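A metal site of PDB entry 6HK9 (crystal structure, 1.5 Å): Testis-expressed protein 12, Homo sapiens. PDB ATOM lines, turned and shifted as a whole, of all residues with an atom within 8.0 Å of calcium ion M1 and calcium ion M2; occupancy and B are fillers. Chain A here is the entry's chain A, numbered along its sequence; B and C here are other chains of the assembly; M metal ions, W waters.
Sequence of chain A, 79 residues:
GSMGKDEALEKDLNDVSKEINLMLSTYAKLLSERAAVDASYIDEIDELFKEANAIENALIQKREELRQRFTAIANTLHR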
ATOM      1  N   ASP A   6     -24.122 -10.008 -13.762  1.00  0.00           N
ATOM      2  CA  ASP A   6     -25.202 -10.509 -12.925  1.00  0.00           C
ATOM      3  C   ASP A   6     -24.741 -11.717 -12.133  1.00  0.00           C
ATOM      4  O   ASP A   6     -25.402 -12.143 -11.193  1.00  0.00           O
ATOM      5  CB  ASP A   6     -26.425 -10.865 -13.761  1.00  0.00           C
ATOM      6  CG  ASP A   6     -26.247 -12.128 -14.558  1.00  0.00           C
ATOM      7  OD1 ASP A   6     -25.122 -12.366 -15.042  1.00  0.00           O
ATOM      8  OD2 ASP A   6     -27.230 -12.883 -14.682  1.00  0.00           O
ATOM      9  N   GLU A   7     -23.613 -12.285 -12.520  1.00  0.00           N
ATOM     10  CA  GLU A   7     -22.959 -13.327 -11.749  1.00  0.00           C
ATOM     11  C   GLU A   7     -21.830 -12.717 -10.930  1.00  0.00           C
ATOM     12  O   GLU A   7     -21.278 -11.663 -11.265  1.00  0.00           O
ATOM     13  CB  GLU A   7     -22.440 -14.441 -12.675  1.00  0.00           C
ATOM     14  CG  GLU A   7     -23.529 -15.073 -13.538  1.00  0.00           C
ATOM     15  CD  GLU A   7     -23.130 -16.431 -14.117  1.00  0.00           C
ATOM     16  OE1 GLU A   7     -22.115 -16.507 -14.840  1.00  0.00           O
ATOM     17  OE2 GLU A   7     -23.850 -17.422 -13.856  1.00  0.00           O
ATOM     18  N   ALA A   8     -21.494 -13.392  -9.838  1.00  0.00           N
ATOM     19  CA  ALA A   8     -20.449 -12.898  -8.951  1.00  0.00           C
ATOM     20  C   ALA A   8     -19.112 -12.821  -9.696  1.00  0.00           C
ATOM     21  O   ALA A   8     -18.881 -13.537 -10.656  1.00  0.00           O
ATOM     22  CB  ALA A   8     -20.307 -13.828  -7.737  1.00  0.00           C
ATOM     23  N   LEU A   9     -18.220 -11.939  -9.220  1.00  0.00           N
ATOM     24  CA  LEU A   9     -16.902 -11.809  -9.843  1.00  0.00           C
ATOM     25  C   LEU A   9     -16.161 -13.140  -9.809  1.00  0.00           C
ATOM     26  O   LEU A   9     -15.416 -13.462 -10.741  1.00  0.00           O
ATOM     27  CB  LEU A   9     -16.088 -10.734  -9.137  1.00  0.00           C
ATOM     28  CG  LEU A   9     -16.533  -9.300  -9.368  1.00  0.00           C
ATOM     29  CD1 LEU A   9     -15.842  -8.335  -8.413  1.00  0.00           C
ATOM     30  CD2 LEU A   9     -16.271  -8.909 -10.823  1.00  0.00           C
ATOM     31  N   GLU A  10     -16.349 -13.909  -8.737  1.00  0.00           N
ATOM     32  CA  GLU A  10     -15.706 -15.227  -8.620  1.00  0.00           C
ATOM     33  C   GLU A  10     -16.197 -16.160  -9.707  1.00  0.00           C
ATOM     34  O   GLU A  10     -15.411 -16.967 -10.230  1.00  0.00           O
ATOM     35  CB  GLU A  10     -16.040 -15.823  -7.252  1.00  0.00           C
ATOM     36  CG  GLU A  10     -15.462 -15.092  -6.081  1.00  0.00           C
ATOM     37  CD  GLU A  10     -16.465 -14.143  -5.408  1.00  0.00           C
ATOM     38  OE1 GLU A  10     -17.354 -13.623  -6.102  1.00  0.00           O
ATOM     39  OE2 GLU A  10     -16.387 -13.912  -4.174  1.00  0.00           O
ATOM     40  N   LYS A  11     -17.492 -16.116 -10.005  1.00  0.00           N
ATOM     41  CA  LYS A  11     -18.053 -16.943 -11.065  1.00  0.00           C
ATOM     42  C   LYS A  11     -17.547 -16.488 -12.413  1.00  0.00           C
ATOM     43  O   LYS A  11     -17.179 -17.305 -13.269  1.00  0.00           O
ATOM     44  CB  LYS A  11     -19.576 -16.862 -11.026  1.00  0.00           C
ATOM     45  CG  LYS A  11     -20.308 -17.532 -12.172  1.00  0.00           C
ATOM     46  CD  LYS A  11     -19.970 -19.017 -12.268  1.00  0.00           C
ATOM     47  CE  LYS A  11     -20.955 -19.771 -13.160  1.00  0.00           C
ATOM     48  NZ  LYS A  11     -21.133 -19.158 -14.512  1.00  0.00           N
ATOM     49  N   ASP A  12     -17.499 -15.163 -12.624  1.00  0.00           N
ATOM     50  CA  ASP A  12     -17.044 -14.652 -13.902  1.00  0.00           C
ATOM     51  C   ASP A  12     -15.562 -14.940 -14.108  1.00  0.00           C
ATOM     52  O   ASP A  12     -15.134 -15.221 -15.227  1.00  0.00           O
ATOM     53  CB  ASP A  12     -17.352 -13.153 -14.024  1.00  0.00           C
ATOM     54  CG  ASP A  12     -18.804 -12.891 -14.336  1.00  0.00           C
ATOM     55  OD1 ASP A  12     -19.520 -13.854 -14.700  1.00  0.00           O
ATOM     56  OD2 ASP A  12     -19.261 -11.721 -14.189  1.00  0.00           O
ATOM     57  N   LEU A  13     -14.773 -14.892 -13.049  1.00  0.00           N
ATOM     58  CA  LEU A  13     -13.363 -15.256 -13.167  1.00  0.00           C
ATOM     59  C   LEU A  13     -13.207 -16.702 -13.604  1.00  0.00           C
ATOM     60  O   LEU A  13     -12.306 -17.040 -14.381  1.00  0.00           O
ATOM     61  CB  LEU A  13     -12.643 -15.022 -11.845  1.00  0.00           C
ATOM     62  CG  LEU A  13     -11.145 -15.324 -11.897  1.00  0.00           C
ATOM     63  CD1 LEU A  13     -10.459 -14.558 -13.033  1.00  0.00           C
ATOM     64  CD2 LEU A  13     -10.539 -14.979 -10.545  1.00  0.00           C
ATOM     65  N   ASN A  14     -14.061 -17.585 -13.096  1.00  0.00           N
ATOM     66  CA  ASN A  14     -13.981 -18.990 -13.454  1.00  0.00           C
ATOM     67  C   ASN A  14     -14.456 -19.198 -14.887  1.00  0.00           C
ATOM     68  O   ASN A  14     -13.888 -20.037 -15.615  1.00  0.00           O
ATOM     69  CB  ASN A  14     -14.814 -19.810 -12.484  1.00  0.00           C
ATOM     70  CG  ASN A  14     -14.477 -21.283 -12.551  1.00  0.00           C
ATOM     71  OD1 ASN A  14     -15.224 -22.075 -13.138  1.00  0.00           O
ATOM     72  ND2 ASN A  14     -13.337 -21.661 -11.972  1.00  0.00           N
ATOM     73  N   ASP A  15     -15.456 -18.438 -15.327  1.00  0.00           N
ATOM     74  CA  ASP A  15     -15.886 -18.559 -16.723  1.00  0.00           C
ATOM     75  C   ASP A  15     -14.785 -18.146 -17.686  1.00  0.00           C
ATOM     76  O   ASP A  15     -14.538 -18.819 -18.696  1.00  0.00           O
ATOM     77  CB  ASP A  15     -17.106 -17.685 -16.977  1.00  0.00           C
ATOM     78  CG  ASP A  15     -18.332 -18.136 -16.212  1.00  0.00           C
ATOM     79  OD1 ASP A  15     -18.449 -19.355 -15.949  1.00  0.00           O
ATOM     80  OD2 ASP A  15     -19.171 -17.268 -15.894  1.00  0.00           O
ATOM     81  N   VAL A  16     -14.139 -17.010 -17.444  1.00  0.00           N
ATOM     82  CA  VAL A  16     -13.134 -16.546 -18.389  1.00  0.00           C
ATOM     83  C   VAL A  16     -11.921 -17.471 -18.361  1.00  0.00           C
ATOM     84  O   VAL A  16     -11.269 -17.698 -19.400  1.00  0.00           O
ATOM     85  CB  VAL A  16     -12.747 -15.073 -18.139  1.00  0.00           C
ATOM     86  CG1 VAL A  16     -12.061 -14.938 -16.798  1.00  0.00           C
ATOM     87  CG2 VAL A  16     -11.841 -14.593 -19.275  1.00  0.00           C
ATOM     88  N   GLU A  19     -12.597 -20.143 -20.763  1.00  0.00           N
ATOM     89  CA  GLU A  19     -12.419 -19.670 -22.125  1.00  0.00           C
ATOM     90  C   GLU A  19     -10.951 -19.640 -22.510  1.00  0.00           C
ATOM     91  O   GLU A  19     -10.586 -20.028 -23.615  1.00  0.00           O
ATOM     92  CB  GLU A  19     -12.995 -18.270 -22.288  1.00  0.00           C
ATOM     93  CG  GLU A  19     -14.511 -18.157 -22.274  1.00  0.00           C
ATOM     94  CD  GLU A  19     -14.979 -16.800 -22.820  1.00  0.00           C
ATOM     95  OE1 GLU A  19     -15.047 -16.662 -24.081  1.00  0.00           O
ATOM     96  OE2 GLU A  19     -15.233 -15.889 -21.996  1.00  0.00           O
ATOM     97  N   ASP B   6     -22.344  -6.773 -14.541  1.00  0.00           N
ATOM     98  CA  ASP B   6     -21.890  -5.564 -13.869  1.00  0.00           C
ATOM     99  C   ASP B   6     -22.372  -4.332 -14.610  1.00  0.00           C
ATOM    100  O   ASP B   6     -22.315  -3.223 -14.092  1.00  0.00           O
ATOM    101  CB  ASP B   6     -20.371  -5.543 -13.745  1.00  0.00           C
ATOM    102  CG  ASP B   6     -19.678  -5.264 -15.050  1.00  0.00           C
ATOM    103  OD1 ASP B   6     -20.170  -5.741 -16.093  1.00  0.00           O
ATOM    104  OD2 ASP B   6     -18.653  -4.556 -15.028  1.00  0.00           O
ATOM    105  N   GLU B   7     -22.842  -4.520 -15.838  1.00  0.00           N
ATOM    106  CA  GLU B   7     -23.493  -3.470 -16.588  1.00  0.00           C
ATOM    107  C   GLU B   7     -25.001  -3.650 -16.492  1.00  0.00           C
ATOM    108  O   GLU B   7     -25.511  -4.752 -16.258  1.00  0.00           O
ATOM    109  CB  GLU B   7     -23.021  -3.476 -18.053  1.00  0.00           C
ATOM    110  CG  GLU B   7     -21.510  -3.320 -18.207  1.00  0.00           C
ATOM    111  CD  GLU B   7     -21.087  -2.891 -19.612  1.00  0.00           C
ATOM    112  OE1 GLU B   7     -21.399  -3.609 -20.585  1.00  0.00           O
ATOM    113  OE2 GLU B   7     -20.433  -1.837 -19.741  1.00  0.00           O
ATOM    114  N   GLU C  51      -9.416  -9.344 -19.749  1.00  0.00           N
ATOM    115  CA  GLU C  51     -10.692  -9.486 -19.067  1.00  0.00           C
ATOM    116  C   GLU C  51     -10.524 -10.287 -17.774  1.00  0.00           C
ATOM    117  O   GLU C  51     -11.080  -9.915 -16.727  1.00  0.00           O
ATOM    118  CB  GLU C  51     -11.702 -10.174 -19.990  1.00  0.00           C
ATOM    119  CG  GLU C  51     -12.872 -10.746 -19.239  1.00  0.00           C
ATOM    120  CD  GLU C  51     -14.071 -11.067 -20.117  1.00  0.00           C
ATOM    121  OE1 GLU C  51     -13.872 -11.415 -21.299  1.00  0.00           O
ATOM    122  OE2 GLU C  51     -15.205 -10.984 -19.588  1.00  0.00           O
ATOM    123  N   ILE C  55     -11.288  -8.932 -13.924  1.00  0.00           N
ATOM    124  CA  ILE C  55     -12.169  -9.620 -12.988  1.00  0.00           C
ATOM    125  C   ILE C  55     -11.411 -10.006 -11.727  1.00  0.00           C
ATOM    126  O   ILE C  55     -11.909  -9.847 -10.604  1.00  0.00           O
ATOM    127  CB  ILE C  55     -12.811 -10.855 -13.643  1.00  0.00           C
ATOM    128  CG1 ILE C  55     -13.680 -10.453 -14.841  1.00  0.00           C
ATOM    129  CG2 ILE C  55     -13.625 -11.622 -12.618  1.00  0.00           C
ATOM    130  CD1 ILE C  55     -14.064 -11.628 -15.699  1.00  0.00           C
ATOM    131  N   LYS C  62     -13.205  -6.706  -4.014  1.00  0.00           N
ATOM    132  CA  LYS C  62     -14.461  -7.097  -3.372  1.00  0.00           C
ATOM    133  C   LYS C  62     -14.202  -7.714  -2.009  1.00  0.00           C
ATOM    134  O   LYS C  62     -14.911  -7.418  -1.026  1.00  0.00           O
ATOM    135  CB  LYS C  62     -15.164  -8.109  -4.263  1.00  0.00           C
ATOM    136  CG  LYS C  62     -16.308  -8.844  -3.555  1.00  0.00           C
ATOM    137  CD  LYS C  62     -16.962  -9.838  -4.493  1.00  0.00           C
ATOM    138  CE  LYS C  62     -18.005 -10.670  -3.781  1.00  0.00           C
ATOM    139  NZ  LYS C  62     -18.677 -11.583  -4.740  1.00  0.00           N
HETATM  140 CA    CA M   1     -20.566 -15.345 -16.240  1.00  0.00          CA
HETATM  141 CA    CA M   2     -21.015  -9.124 -11.131  1.00  0.00          CA
HETATM  142 CA    CA M   3     -26.498  -6.473 -14.646  1.00  0.00          CA
HETATM  143  O   HOH W   1     -22.129 -13.722 -16.717  1.00  0.00           O
HETATM  144  O   HOH W   2     -21.240 -16.161 -18.178  1.00  0.00           O
HETATM  145  O   HOH W   3     -18.965 -14.620 -17.627  1.00  0.00           O
HETATM  146  O   HOH W   4     -19.307  -9.751 -12.618  1.00  0.00           O
HETATM  147  O   HOH W   5     -22.324  -8.871 -12.948  1.00  0.00           O
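Calcium ion M2 is bound by water W5, water W4 and the backbone carbonyl oxygen of Glu 7 of chain A. Calcium ion M2 has three donor atoms within binding distance.
NZ of Lys 11 lies within salt-bridge range of OE2 of Glu 7 of chain A, 3.3 Å away. The side-chain amino group of Lys 11 is in salt-bridge range of the side-chain carboxylate of Asp 15, 3.1 Å away.
The nearest printed residue that does not touch calcium ion M1 is Lys 11 (4.2 Å).
Calcium ion M1 is bound by water W2 (2.2 Å), water W3 (2.2 Å), water W1 (2.3 Å), the side-chain carboxylate (OD1) of Asp 12 (2.4 Å), the side-chain carboxylate (OE1) of Glu 7 of chain A (2.4 Å) and the side-chain carboxylate (OD2) of Asp 15 (2.4 Å). Calcium ion M1 has six donor atoms within binding distance.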
